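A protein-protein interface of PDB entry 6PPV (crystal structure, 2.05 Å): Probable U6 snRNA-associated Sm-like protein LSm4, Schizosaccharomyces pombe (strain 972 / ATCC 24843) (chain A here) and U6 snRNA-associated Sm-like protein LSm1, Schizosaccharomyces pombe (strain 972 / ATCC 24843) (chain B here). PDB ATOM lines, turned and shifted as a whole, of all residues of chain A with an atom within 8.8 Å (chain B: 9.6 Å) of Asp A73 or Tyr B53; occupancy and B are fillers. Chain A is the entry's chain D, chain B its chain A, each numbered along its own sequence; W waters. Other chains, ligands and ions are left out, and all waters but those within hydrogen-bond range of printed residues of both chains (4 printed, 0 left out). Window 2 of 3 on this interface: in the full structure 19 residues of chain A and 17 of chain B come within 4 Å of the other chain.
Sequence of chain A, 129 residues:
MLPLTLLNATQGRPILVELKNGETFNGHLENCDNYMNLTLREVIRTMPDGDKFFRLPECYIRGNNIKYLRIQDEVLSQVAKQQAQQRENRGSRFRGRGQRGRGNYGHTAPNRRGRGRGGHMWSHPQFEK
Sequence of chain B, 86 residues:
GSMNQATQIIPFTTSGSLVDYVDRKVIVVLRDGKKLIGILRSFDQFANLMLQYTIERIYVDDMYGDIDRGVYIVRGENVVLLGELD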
ATOM      1  N   LEU A   6      11.355 -19.654  -9.036  1.00  0.00           N
ATOM      2  CA  LEU A   6      12.049 -19.485 -10.308  1.00  0.00           C
ATOM      3  C   LEU A   6      12.282 -18.010 -10.616  1.00  0.00           C
ATOM      4  O   LEU A   6      13.381 -17.611 -11.029  1.00  0.00           O
ATOM      5  CB  LEU A   6      11.243 -20.145 -11.429  1.00  0.00           C
ATOM      6  CG  LEU A   6      11.829 -19.983 -12.823  1.00  0.00           C
ATOM      7  CD1 LEU A   6      13.228 -20.598 -12.868  1.00  0.00           C
ATOM      8  CD2 LEU A   6      10.916 -20.614 -13.873  1.00  0.00           C
ATOM      9  N   PRO A  14      18.482 -12.206 -18.303  1.00  0.00           N
ATOM     10  CA  PRO A  14      17.456 -11.634 -19.183  1.00  0.00           C
ATOM     11  C   PRO A  14      16.069 -12.189 -18.884  1.00  0.00           C
ATOM     12  O   PRO A  14      15.906 -13.303 -18.378  1.00  0.00           O
ATOM     13  CB  PRO A  14      17.929 -12.026 -20.592  1.00  0.00           C
ATOM     14  CG  PRO A  14      19.053 -13.014 -20.394  1.00  0.00           C
ATOM     15  CD  PRO A  14      19.637 -12.727 -19.056  1.00  0.00           C
ATOM     16  N   ARG A  70       8.619 -14.525 -19.680  1.00  0.00           N
ATOM     17  CA  ARG A  70       9.377 -15.552 -20.378  1.00  0.00           C
ATOM     18  C   ARG A  70      10.832 -15.482 -19.942  1.00  0.00           C
ATOM     19  O   ARG A  70      11.396 -14.389 -19.779  1.00  0.00           O
ATOM     20  CB  ARG A  70       9.265 -15.402 -21.893  1.00  0.00           C
ATOM     21  CG  ARG A  70       7.909 -15.803 -22.442  1.00  0.00           C
ATOM     22  CD  ARG A  70       7.813 -15.574 -23.952  1.00  0.00           C
ATOM     23  NE  ARG A  70       8.845 -16.298 -24.682  1.00  0.00           N
ATOM     24  CZ  ARG A  70       9.420 -15.863 -25.800  1.00  0.00           C
ATOM     25  NH1 ARG A  70       9.055 -14.696 -26.315  1.00  0.00           N
ATOM     26  NH2 ARG A  70      10.362 -16.590 -26.399  1.00  0.00           N
ATOM     27  N   ILE A  71      11.426 -16.658 -19.731  1.00  0.00           N
ATOM     28  CA  ILE A  71      12.823 -16.778 -19.344  1.00  0.00           C
ATOM     29  C   ILE A  71      13.489 -17.860 -20.189  1.00  0.00           C
ATOM     30  O   ILE A  71      12.830 -18.719 -20.784  1.00  0.00           O
ATOM     31  CB  ILE A  71      12.992 -17.086 -17.840  1.00  0.00           C
ATOM     32  CG1 ILE A  71      12.775 -18.562 -17.573  1.00  0.00           C
ATOM     33  CG2 ILE A  71      11.991 -16.284 -16.986  1.00  0.00           C
ATOM     34  CD1 ILE A  71      12.973 -18.928 -16.126  1.00  0.00           C
ATOM     35  N   GLN A  72      14.817 -17.802 -20.241  1.00  0.00           N
ATOM     36  CA  GLN A  72      15.593 -18.799 -20.970  1.00  0.00           C
ATOM     37  C   GLN A  72      15.479 -20.163 -20.295  1.00  0.00           C
ATOM     38  O   GLN A  72      15.520 -20.270 -19.067  1.00  0.00           O
ATOM     39  CB  GLN A  72      17.062 -18.374 -21.045  1.00  0.00           C
ATOM     40  CG  GLN A  72      17.285 -16.951 -21.569  1.00  0.00           C
ATOM     41  CD  GLN A  72      18.658 -16.381 -21.197  1.00  0.00           C
ATOM     42  OE1 GLN A  72      19.018 -16.308 -20.020  1.00  0.00           O
ATOM     43  NE2 GLN A  72      19.425 -15.975 -22.206  1.00  0.00           N
ATOM     44  N   ASP A  73      15.331 -21.211 -21.111  1.00  0.00           N
ATOM     45  CA  ASP A  73      15.295 -22.574 -20.580  1.00  0.00           C
ATOM     46  C   ASP A  73      16.546 -22.891 -19.763  1.00  0.00           C
ATOM     47  O   ASP A  73      16.473 -23.577 -18.730  1.00  0.00           O
ATOM     48  CB  ASP A  73      15.142 -23.567 -21.727  1.00  0.00           C
ATOM     49  CG  ASP A  73      15.033 -24.989 -21.246  1.00  0.00           C
ATOM     50  OD1 ASP A  73      13.931 -25.390 -20.817  1.00  0.00           O
ATOM     51  OD2 ASP A  73      16.053 -25.709 -21.286  1.00  0.00           O
ATOM     52  N   GLU A  74      17.699 -22.383 -20.213  1.00  0.00           N
ATOM     53  CA  GLU A  74      18.967 -22.608 -19.525  1.00  0.00           C
ATOM     54  C   GLU A  74      18.884 -22.203 -18.062  1.00  0.00           C
ATOM     55  O   GLU A  74      19.481 -22.851 -17.193  1.00  0.00           O
ATOM     56  CB  GLU A  74      20.087 -21.827 -20.225  1.00  0.00           C
ATOM     57  CG  GLU A  74      20.354 -22.232 -21.678  1.00  0.00           C
ATOM     58  CD  GLU A  74      19.227 -21.846 -22.634  1.00  0.00           C
ATOM     59  OE1 GLU A  74      18.385 -20.999 -22.262  1.00  0.00           O
ATOM     60  OE2 GLU A  74      19.174 -22.402 -23.754  1.00  0.00           O
ATOM     61  N   VAL A  75      18.159 -21.117 -17.775  1.00  0.00           N
ATOM     62  CA  VAL A  75      17.987 -20.665 -16.398  1.00  0.00           C
ATOM     63  C   VAL A  75      17.280 -21.729 -15.574  1.00  0.00           C
ATOM     64  O   VAL A  75      17.668 -22.015 -14.435  1.00  0.00           O
ATOM     65  CB  VAL A  75      17.214 -19.333 -16.368  1.00  0.00           C
ATOM     66  CG1 VAL A  75      16.878 -18.945 -14.932  1.00  0.00           C
ATOM     67  CG2 VAL A  75      18.001 -18.232 -17.083  1.00  0.00           C
ATOM     68  N   LEU A  76      16.221 -22.319 -16.129  1.00  0.00           N
ATOM     69  CA  LEU A  76      15.494 -23.351 -15.400  1.00  0.00           C
ATOM     70  C   LEU A  76      16.382 -24.565 -15.151  1.00  0.00           C
ATOM     71  O   LEU A  76      16.358 -25.152 -14.059  1.00  0.00           O
ATOM     72  CB  LEU A  76      14.225 -23.733 -16.167  1.00  0.00           C
ATOM     73  CG  LEU A  76      13.272 -24.676 -15.437  1.00  0.00           C
ATOM     74  CD1 LEU A  76      13.064 -24.201 -14.000  1.00  0.00           C
ATOM     75  CD2 LEU A  76      11.942 -24.792 -16.181  1.00  0.00           C
ATOM     76  N   SER A  77      17.200 -24.933 -16.144  1.00  0.00           N
ATOM     77  CA  SER A  77      18.150 -26.030 -15.948  1.00  0.00           C
ATOM     78  C   SER A  77      19.132 -25.719 -14.817  1.00  0.00           C
ATOM     79  O   SER A  77      19.271 -26.497 -13.864  1.00  0.00           O
ATOM     80  CB  SER A  77      18.901 -26.301 -17.249  1.00  0.00           C
ATOM     81  OG  SER A  77      18.035 -26.179 -18.366  1.00  0.00           O
ATOM     82  N   GLN A  78      19.814 -24.575 -14.904  1.00  0.00           N
ATOM     83  CA  GLN A  78      20.846 -24.221 -13.937  1.00  0.00           C
ATOM     84  C   GLN A  78      20.282 -23.959 -12.546  1.00  0.00           C
ATOM     85  O   GLN A  78      21.028 -24.043 -11.564  1.00  0.00           O
ATOM     86  CB  GLN A  78      21.618 -22.995 -14.426  1.00  0.00           C
ATOM     87  N   VAL A  79      18.993 -23.630 -12.440  1.00  0.00           N
ATOM     88  CA  VAL A  79      18.374 -23.492 -11.127  1.00  0.00           C
ATOM     89  C   VAL A  79      18.009 -24.858 -10.563  1.00  0.00           C
ATOM     90  O   VAL A  79      18.156 -25.103  -9.360  1.00  0.00           O
ATOM     91  CB  VAL A  79      17.150 -22.558 -11.208  1.00  0.00           C
ATOM     92  N   ALA A  80      17.532 -25.770 -11.419  1.00  0.00           N
ATOM     93  CA  ALA A  80      17.306 -27.141 -10.971  1.00  0.00           C
ATOM     94  C   ALA A  80      18.595 -27.769 -10.450  1.00  0.00           C
ATOM     95  O   ALA A  80      18.589 -28.456  -9.421  1.00  0.00           O
ATOM     96  CB  ALA A  80      16.721 -27.982 -12.105  1.00  0.00           C
ATOM     97  N   ASP B  23       4.128 -32.111 -14.739  1.00  0.00           N
ATOM     98  CA  ASP B  23       4.954 -32.888 -15.663  1.00  0.00           C
ATOM     99  C   ASP B  23       4.159 -33.466 -16.826  1.00  0.00           C
ATOM    100  O   ASP B  23       4.662 -34.352 -17.525  1.00  0.00           O
ATOM    101  CB  ASP B  23       5.726 -34.000 -14.938  1.00  0.00           C
ATOM    102  CG  ASP B  23       6.778 -33.439 -13.987  1.00  0.00           C
ATOM    103  OD1 ASP B  23       7.417 -32.438 -14.372  1.00  0.00           O
ATOM    104  OD2 ASP B  23       6.949 -33.966 -12.860  1.00  0.00           O
ATOM    105  N   ARG B  24       2.940 -32.984 -17.064  1.00  0.00           N
ATOM    106  CA  ARG B  24       2.142 -33.376 -18.218  1.00  0.00           C
ATOM    107  C   ARG B  24       2.074 -32.236 -19.230  1.00  0.00           C
ATOM    108  O   ARG B  24       2.262 -31.061 -18.898  1.00  0.00           O
ATOM    109  CB  ARG B  24       0.722 -33.773 -17.795  1.00  0.00           C
ATOM    110  N   LYS B  25       1.793 -32.599 -20.476  1.00  0.00           N
ATOM    111  CA  LYS B  25       1.567 -31.613 -21.519  1.00  0.00           C
ATOM    112  C   LYS B  25       0.163 -31.027 -21.387  1.00  0.00           C
ATOM    113  O   LYS B  25      -0.824 -31.767 -21.276  1.00  0.00           O
ATOM    114  CB  LYS B  25       1.747 -32.245 -22.892  1.00  0.00           C
ATOM    115  CG  LYS B  25       1.736 -31.267 -24.058  1.00  0.00           C
ATOM    116  CD  LYS B  25       2.293 -31.940 -25.309  1.00  0.00           C
ATOM    117  CE  LYS B  25       1.507 -31.574 -26.548  1.00  0.00           C
ATOM    118  NZ  LYS B  25       1.829 -32.501 -27.674  1.00  0.00           N
ATOM    119  N   VAL B  26       0.079 -29.693 -21.409  1.00  0.00           N
ATOM    120  CA  VAL B  26      -1.171 -28.975 -21.231  1.00  0.00           C
ATOM    121  C   VAL B  26      -1.287 -27.867 -22.268  1.00  0.00           C
ATOM    122  O   VAL B  26      -0.298 -27.365 -22.812  1.00  0.00           O
ATOM    123  CB  VAL B  26      -1.303 -28.368 -19.819  1.00  0.00           C
ATOM    124  CG1 VAL B  26      -1.186 -29.441 -18.750  1.00  0.00           C
ATOM    125  CG2 VAL B  26      -0.257 -27.285 -19.617  1.00  0.00           C
ATOM    126  N   LEU B  36      -1.236 -21.415 -25.220  1.00  0.00           N
ATOM    127  CA  LEU B  36       0.102 -21.906 -24.942  1.00  0.00           C
ATOM    128  C   LEU B  36       0.039 -23.416 -24.764  1.00  0.00           C
ATOM    129  O   LEU B  36      -0.863 -23.925 -24.102  1.00  0.00           O
ATOM    130  CB  LEU B  36       0.673 -21.260 -23.677  1.00  0.00           C
ATOM    131  CG  LEU B  36       0.716 -19.729 -23.609  1.00  0.00           C
ATOM    132  CD1 LEU B  36       1.312 -19.291 -22.271  1.00  0.00           C
ATOM    133  CD2 LEU B  36       1.530 -19.160 -24.780  1.00  0.00           C
ATOM    134  N   ILE B  37       0.989 -24.141 -25.347  1.00  0.00           N
ATOM    135  CA  ILE B  37       1.038 -25.590 -25.197  1.00  0.00           C
ATOM    136  C   ILE B  37       2.424 -25.968 -24.703  1.00  0.00           C
ATOM    137  O   ILE B  37       3.419 -25.728 -25.394  1.00  0.00           O
ATOM    138  CB  ILE B  37       0.699 -26.322 -26.502  1.00  0.00           C
ATOM    139  CG1 ILE B  37      -0.746 -26.030 -26.893  1.00  0.00           C
ATOM    140  CG2 ILE B  37       0.907 -27.827 -26.343  1.00  0.00           C
ATOM    141  CD1 ILE B  37      -1.127 -26.567 -28.236  1.00  0.00           C
ATOM    142  N   GLY B  38       2.490 -26.549 -23.513  1.00  0.00           N
ATOM    143  CA  GLY B  38       3.778 -26.898 -22.961  1.00  0.00           C
ATOM    144  C   GLY B  38       3.654 -27.856 -21.798  1.00  0.00           C
ATOM    145  O   GLY B  38       2.570 -28.357 -21.490  1.00  0.00           O
ATOM    146  N   ILE B  39       4.783 -28.101 -21.143  1.00  0.00           N
ATOM    147  CA  ILE B  39       4.829 -29.006 -19.999  1.00  0.00           C
ATOM    148  C   ILE B  39       4.637 -28.199 -18.726  1.00  0.00           C
ATOM    149  O   ILE B  39       5.433 -27.305 -18.417  1.00  0.00           O
ATOM    150  CB  ILE B  39       6.149 -29.788 -19.948  1.00  0.00           C
ATOM    151  CG1 ILE B  39       6.412 -30.477 -21.288  1.00  0.00           C
ATOM    152  CG2 ILE B  39       6.115 -30.778 -18.790  1.00  0.00           C
ATOM    153  CD1 ILE B  39       5.254 -31.334 -21.783  1.00  0.00           C
ATOM    154  N   LEU B  40       3.594 -28.522 -17.973  1.00  0.00           N
ATOM    155  CA  LEU B  40       3.387 -27.860 -16.699  1.00  0.00           C
ATOM    156  C   LEU B  40       4.428 -28.347 -15.702  1.00  0.00           C
ATOM    157  O   LEU B  40       4.454 -29.531 -15.354  1.00  0.00           O
ATOM    158  CB  LEU B  40       1.981 -28.123 -16.176  1.00  0.00           C
ATOM    159  CG  LEU B  40       1.724 -27.426 -14.838  1.00  0.00           C
ATOM    160  CD1 LEU B  40       1.741 -25.894 -15.015  1.00  0.00           C
ATOM    161  CD2 LEU B  40       0.423 -27.911 -14.224  1.00  0.00           C
ATOM    162  N   ARG B  41       5.290 -27.441 -15.249  1.00  0.00           N
ATOM    163  CA  ARG B  41       6.274 -27.760 -14.221  1.00  0.00           C
ATOM    164  C   ARG B  41       5.842 -27.364 -12.819  1.00  0.00           C
ATOM    165  O   ARG B  41       6.171 -28.080 -11.863  1.00  0.00           O
ATOM    166  CB  ARG B  41       7.618 -27.094 -14.526  1.00  0.00           C
ATOM    167  CG  ARG B  41       8.297 -27.641 -15.766  1.00  0.00           C
ATOM    168  CD  ARG B  41       8.494 -29.166 -15.717  1.00  0.00           C
ATOM    169  NE  ARG B  41       9.385 -29.602 -16.799  1.00  0.00           N
ATOM    170  CZ  ARG B  41       9.634 -30.869 -17.107  1.00  0.00           C
ATOM    171  NH1 ARG B  41       9.046 -31.845 -16.419  1.00  0.00           N
ATOM    172  NH2 ARG B  41      10.471 -31.159 -18.102  1.00  0.00           N
ATOM    173  N   MET B  50       4.031 -22.319 -14.203  1.00  0.00           N
ATOM    174  CA  MET B  50       5.348 -22.349 -14.816  1.00  0.00           C
ATOM    175  C   MET B  50       5.375 -23.510 -15.794  1.00  0.00           C
ATOM    176  O   MET B  50       5.191 -24.670 -15.386  1.00  0.00           O
ATOM    177  CB  MET B  50       6.468 -22.472 -13.781  1.00  0.00           C
ATOM    178  CG  MET B  50       7.830 -22.186 -14.390  1.00  0.00           C
ATOM    179  SD  MET B  50       8.712 -23.644 -14.991  1.00  0.00           S
ATOM    180  CE  MET B  50       9.461 -24.199 -13.459  1.00  0.00           C
ATOM    181  N   LEU B  51       5.605 -23.170 -17.070  1.00  0.00           N
ATOM    182  CA  LEU B  51       5.576 -24.075 -18.209  1.00  0.00           C
ATOM    183  C   LEU B  51       6.936 -24.115 -18.894  1.00  0.00           C
ATOM    184  O   LEU B  51       7.574 -23.067 -19.096  1.00  0.00           O
ATOM    185  CB  LEU B  51       4.554 -23.636 -19.251  1.00  0.00           C
ATOM    186  CG  LEU B  51       3.120 -23.274 -18.885  1.00  0.00           C
ATOM    187  CD1 LEU B  51       2.531 -22.475 -20.038  1.00  0.00           C
ATOM    188  CD2 LEU B  51       2.314 -24.541 -18.635  1.00  0.00           C
ATOM    189  N   GLN B  52       7.339 -25.319 -19.302  1.00  0.00           N
ATOM    190  CA  GLN B  52       8.586 -25.548 -20.023  1.00  0.00           C
ATOM    191  C   GLN B  52       8.308 -26.126 -21.409  1.00  0.00           C
ATOM    192  O   GLN B  52       7.292 -26.801 -21.627  1.00  0.00           O
ATOM    193  CB  GLN B  52       9.506 -26.494 -19.242  1.00  0.00           C
ATOM    194  CG  GLN B  52      10.902 -26.655 -19.868  1.00  0.00           C
ATOM    195  CD  GLN B  52      11.846 -27.470 -19.013  1.00  0.00           C
ATOM    196  OE1 GLN B  52      11.428 -28.215 -18.116  1.00  0.00           O
ATOM    197  NE2 GLN B  52      13.136 -27.330 -19.283  1.00  0.00           N
ATOM    198  N   TYR B  53       9.235 -25.863 -22.339  1.00  0.00           N
ATOM    199  CA  TYR B  53       9.129 -26.296 -23.736  1.00  0.00           C
ATOM    200  C   TYR B  53       7.815 -25.835 -24.353  1.00  0.00           C
ATOM    201  O   TYR B  53       7.103 -26.593 -25.009  1.00  0.00           O
ATOM    202  CB  TYR B  53       9.280 -27.818 -23.874  1.00  0.00           C
ATOM    203  CG  TYR B  53      10.449 -28.404 -23.114  1.00  0.00           C
ATOM    204  CD1 TYR B  53      11.745 -27.981 -23.365  1.00  0.00           C
ATOM    205  CD2 TYR B  53      10.251 -29.384 -22.147  1.00  0.00           C
ATOM    206  CE1 TYR B  53      12.815 -28.506 -22.670  1.00  0.00           C
ATOM    207  CE2 TYR B  53      11.314 -29.917 -21.440  1.00  0.00           C
ATOM    208  CZ  TYR B  53      12.598 -29.476 -21.708  1.00  0.00           C
ATOM    209  OH  TYR B  53      13.670 -30.004 -21.016  1.00  0.00           O
ATOM    210  N   THR B  54       7.499 -24.563 -24.159  1.00  0.00           N
ATOM    211  CA  THR B  54       6.200 -24.050 -24.547  1.00  0.00           C
ATOM    212  C   THR B  54       6.204 -23.575 -25.998  1.00  0.00           C
ATOM    213  O   THR B  54       7.162 -22.956 -26.471  1.00  0.00           O
ATOM    214  CB  THR B  54       5.784 -22.907 -23.614  1.00  0.00           C
ATOM    215  OG1 THR B  54       6.099 -23.258 -22.262  1.00  0.00           O
ATOM    216  CG2 THR B  54       4.286 -22.646 -23.711  1.00  0.00           C
ATOM    217  N   ILE B  55       5.130 -23.879 -26.707  1.00  0.00           N
ATOM    218  CA  ILE B  55       4.858 -23.245 -27.985  1.00  0.00           C
ATOM    219  C   ILE B  55       3.625 -22.370 -27.809  1.00  0.00           C
ATOM    220  O   ILE B  55       2.765 -22.637 -26.963  1.00  0.00           O
ATOM    221  CB  ILE B  55       4.660 -24.268 -29.122  1.00  0.00           C
ATOM    222  CG1 ILE B  55       3.483 -25.191 -28.812  1.00  0.00           C
ATOM    223  CG2 ILE B  55       5.947 -25.064 -29.356  1.00  0.00           C
ATOM    224  CD1 ILE B  55       2.318 -25.031 -29.768  1.00  0.00           C
ATOM    225  N   GLU B  56       3.569 -21.290 -28.575  1.00  0.00           N
ATOM    226  CA  GLU B  56       2.358 -20.501 -28.718  1.00  0.00           C
ATOM    227  C   GLU B  56       1.716 -20.898 -30.041  1.00  0.00           C
ATOM    228  O   GLU B  56       2.365 -20.841 -31.094  1.00  0.00           O
ATOM    229  CB  GLU B  56       2.662 -19.006 -28.677  1.00  0.00           C
ATOM    230  CG  GLU B  56       1.422 -18.133 -28.603  1.00  0.00           C
ATOM    231  CD  GLU B  56       1.748 -16.657 -28.692  1.00  0.00           C
ATOM    232  OE1 GLU B  56       0.867 -15.886 -29.117  1.00  0.00           O
ATOM    233  OE2 GLU B  56       2.890 -16.267 -28.352  1.00  0.00           O
ATOM    234  N   ASP B  66       2.654 -22.674 -35.180  1.00  0.00           N
ATOM    235  CA  ASP B  66       3.287 -22.701 -33.871  1.00  0.00           C
ATOM    236  C   ASP B  66       4.509 -21.795 -33.843  1.00  0.00           C
ATOM    237  O   ASP B  66       5.141 -21.546 -34.872  1.00  0.00           O
ATOM    238  CB  ASP B  66       3.687 -24.128 -33.486  1.00  0.00           C
ATOM    239  CG  ASP B  66       2.480 -25.012 -33.212  1.00  0.00           C
ATOM    240  OD1 ASP B  66       1.348 -24.468 -33.135  1.00  0.00           O
ATOM    241  OD2 ASP B  66       2.660 -26.244 -33.083  1.00  0.00           O
ATOM    242  N   ILE B  67       4.812 -21.284 -32.648  1.00  0.00           N
ATOM    243  CA  ILE B  67       6.010 -20.490 -32.379  1.00  0.00           C
ATOM    244  C   ILE B  67       6.645 -21.037 -31.113  1.00  0.00           C
ATOM    245  O   ILE B  67       5.983 -21.098 -30.069  1.00  0.00           O
ATOM    246  CB  ILE B  67       5.691 -18.995 -32.187  1.00  0.00           C
ATOM    247  CG1 ILE B  67       4.966 -18.420 -33.402  1.00  0.00           C
ATOM    248  CG2 ILE B  67       6.966 -18.202 -31.871  1.00  0.00           C
ATOM    249  CD1 ILE B  67       4.315 -17.090 -33.108  1.00  0.00           C
ATOM    250  N   ASP B  68       7.922 -21.412 -31.190  1.00  0.00           N
ATOM    251  CA  ASP B  68       8.656 -21.815 -29.994  1.00  0.00           C
ATOM    252  C   ASP B  68       8.828 -20.627 -29.050  1.00  0.00           C
ATOM    253  O   ASP B  68       9.114 -19.507 -29.484  1.00  0.00           O
ATOM    254  CB  ASP B  68      10.024 -22.388 -30.370  1.00  0.00           C
ATOM    255  CG  ASP B  68       9.918 -23.626 -31.238  1.00  0.00           C
ATOM    256  OD1 ASP B  68       9.043 -24.473 -30.971  1.00  0.00           O
ATOM    257  OD2 ASP B  68      10.709 -23.754 -32.196  1.00  0.00           O
ATOM    258  N   ARG B  69       8.664 -20.873 -27.746  1.00  0.00           N
ATOM    259  CA  ARG B  69       8.649 -19.794 -26.764  1.00  0.00           C
ATOM    260  C   ARG B  69       9.467 -20.060 -25.515  1.00  0.00           C
ATOM    261  O   ARG B  69       9.716 -19.111 -24.761  1.00  0.00           O
ATOM    262  CB  ARG B  69       7.208 -19.486 -26.329  1.00  0.00           C
ATOM    263  CG  ARG B  69       6.341 -18.912 -27.413  1.00  0.00           C
ATOM    264  CD  ARG B  69       6.902 -17.588 -27.877  1.00  0.00           C
ATOM    265  NE  ARG B  69       5.895 -16.780 -28.539  1.00  0.00           N
ATOM    266  CZ  ARG B  69       6.156 -15.670 -29.222  1.00  0.00           C
ATOM    267  NH1 ARG B  69       5.165 -14.993 -29.791  1.00  0.00           N
ATOM    268  NH2 ARG B  69       7.404 -15.238 -29.341  1.00  0.00           N
ATOM    269  N   GLY B  70       9.846 -21.295 -25.222  1.00  0.00           N
ATOM    270  CA  GLY B  70      10.644 -21.532 -24.042  1.00  0.00           C
ATOM    271  C   GLY B  70       9.846 -21.675 -22.766  1.00  0.00           C
ATOM    272  O   GLY B  70       8.840 -22.389 -22.717  1.00  0.00           O
ATOM    273  N   VAL B  71      10.308 -21.010 -21.715  1.00  0.00           N
ATOM    274  CA  VAL B  71       9.724 -21.126 -20.388  1.00  0.00           C
ATOM    275  C   VAL B  71       8.815 -19.924 -20.156  1.00  0.00           C
ATOM    276  O   VAL B  71       9.196 -18.785 -20.456  1.00  0.00           O
ATOM    277  CB  VAL B  71      10.823 -21.207 -19.317  1.00  0.00           C
ATOM    278  CG1 VAL B  71      10.224 -21.116 -17.918  1.00  0.00           C
ATOM    279  CG2 VAL B  71      11.647 -22.496 -19.490  1.00  0.00           C
ATOM    280  N   TYR B  72       7.615 -20.174 -19.630  1.00  0.00           N
ATOM    281  CA  TYR B  72       6.712 -19.119 -19.176  1.00  0.00           C
ATOM    282  C   TYR B  72       6.495 -19.211 -17.673  1.00  0.00           C
ATOM    283  O   TYR B  72       6.371 -20.312 -17.122  1.00  0.00           O
ATOM    284  CB  TYR B  72       5.323 -19.207 -19.813  1.00  0.00           C
ATOM    285  CG  TYR B  72       5.181 -18.742 -21.231  1.00  0.00           C
ATOM    286  CD1 TYR B  72       5.404 -19.611 -22.281  1.00  0.00           C
ATOM    287  CD2 TYR B  72       4.754 -17.453 -21.521  1.00  0.00           C
ATOM    288  CE1 TYR B  72       5.243 -19.209 -23.581  1.00  0.00           C
ATOM    289  CE2 TYR B  72       4.591 -17.036 -22.822  1.00  0.00           C
ATOM    290  CZ  TYR B  72       4.838 -17.926 -23.852  1.00  0.00           C
ATOM    291  OH  TYR B  72       4.681 -17.537 -25.158  1.00  0.00           O
HETATM  292  O   HOH W   1      15.889 -28.402 -20.588  1.00  0.00           O
HETATM  293  O   HOH W   2       9.727 -16.466 -29.311  1.00  0.00           O
HETATM  294  O   HOH W   3      11.998 -18.928 -26.911  1.00  0.00           O
HETATM  295  O   HOH W   4      11.674 -24.591 -22.306  1.00  0.00           O
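Met B50 touches Leu A6 (CG to CD2, 3.5 Å).
Val B71 touches Arg A70.
CG of Arg A70 touches CE2 of Tyr B72, 3.6 Å away.
Tyr B53 touches Asp A73.
Asp A73 touches Val B71 (CA to CG2, 3.8 Å).
Met B50 touches Leu A76.
Leu A76 touches Gln B52 (CD2 to CD, 3.9 Å).
N of Tyr B72 is in hydrogen-bond range of O of Leu B51 (2.9 Å).
The backbone NH of Ile B39 is in hydrogen-bond range of the backbone carbonyl oxygen of Gln B52, 2.9 Å away.
The backbone NH (N) of Arg B41 sits at hydrogen-bond distance from the backbone carbonyl oxygen (O) of Met B50, at 2.8 Å.
The backbone carbonyl oxygen (O) of Asp A73 is in hydrogen-bond range of the side-chain hydroxyl (OG) of Ser A77 (3.1 Å).
The side-chain hydroxyl (OH) of Tyr B53 is in hydrogen-bond range of the side-chain amide nitrogen (NE2) of Gln B52 (3.2 Å).
The backbone carbonyl oxygen (O) of Thr B54 sits at hydrogen-bond distance from the backbone NH (N) of Arg B69 (2.9 Å).
Of the 24 printed residues of chain B, 6 touch a printed residue of chain A.
Hydrophobic or aromatic side chains of chain B that line the printed part of chain A: Met B50, Tyr B53, Val B71 and Tyr B72.
Hydrophobic or aromatic side chains of chain A within 4 Å of the printed part of chain B: Leu A6, Ile A71 and Leu A76.
Printed residues of chain B within 4 Å of Leu A6: Met B50.
Of the printed residues of chain B, Arg A70 touches Arg B69, Val B71 and Tyr B72.
Of the printed residues of chain B, Ile A71 touches Val B71.
Asp A73 touches just these residues of chain B: Gln B52, Tyr B53 and Val B71.
Of chain A, only Asp A73 (2.6 Å) and Leu A76 (3.9 Å) come within 4 Å of Gln B52.
Of chain A, only Asp A73 (3.8 Å) comes within 4 Å of Tyr B53.
Ile B55 touches none of the printed residues of chain A.
Printed residues of chain A within 4 Å of Arg B69: Arg A70 (2.9 Å).
Of the printed residues of chain A, Tyr B72 touches Arg A70.
The nearest residue of chain B that does not touch Asp A73 is Gly B70 (5.5 Å).
The nearest printed residue of chain A that does not touch Met B50 is Ile A71 (6.3 Å).
Water W2 lies within hydrogen-bond range of NH2 of Arg B69, NH2 of Arg A70 and O of Asp B68.
Water W4 bridges the backbone NH (N) of Tyr B53 (2.8 Å) and the side-chain carboxylate (OD1) of Asp A73 (2.8 Å).
Water W1 lies within hydrogen-bond range of the side-chain hydroxyl (OH) of Tyr B53, the side-chain carboxylate (OD2) of Asp A73 and the side-chain amide nitrogen (NE2) of Gln B52.
Water W3 lies within hydrogen-bond range of the guanidinium group of Arg A70 (2.9 Å) and the backbone carbonyl oxygen of Arg B69 (3.1 Å).
NE of Arg A70 sits at hydrogen-bond distance from O of Arg B69, 2.9 Å away.
The side-chain carboxylate (OD1) of Asp A73 is in hydrogen-bond range of the side-chain amide nitrogen (NE2) of Gln B52 (2.6 Å).
The backbone carbonyl oxygen (O) of Val B71 lies within hydrogen-bond range of the backbone NH (N) of Ile A71 (3.2 Å).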
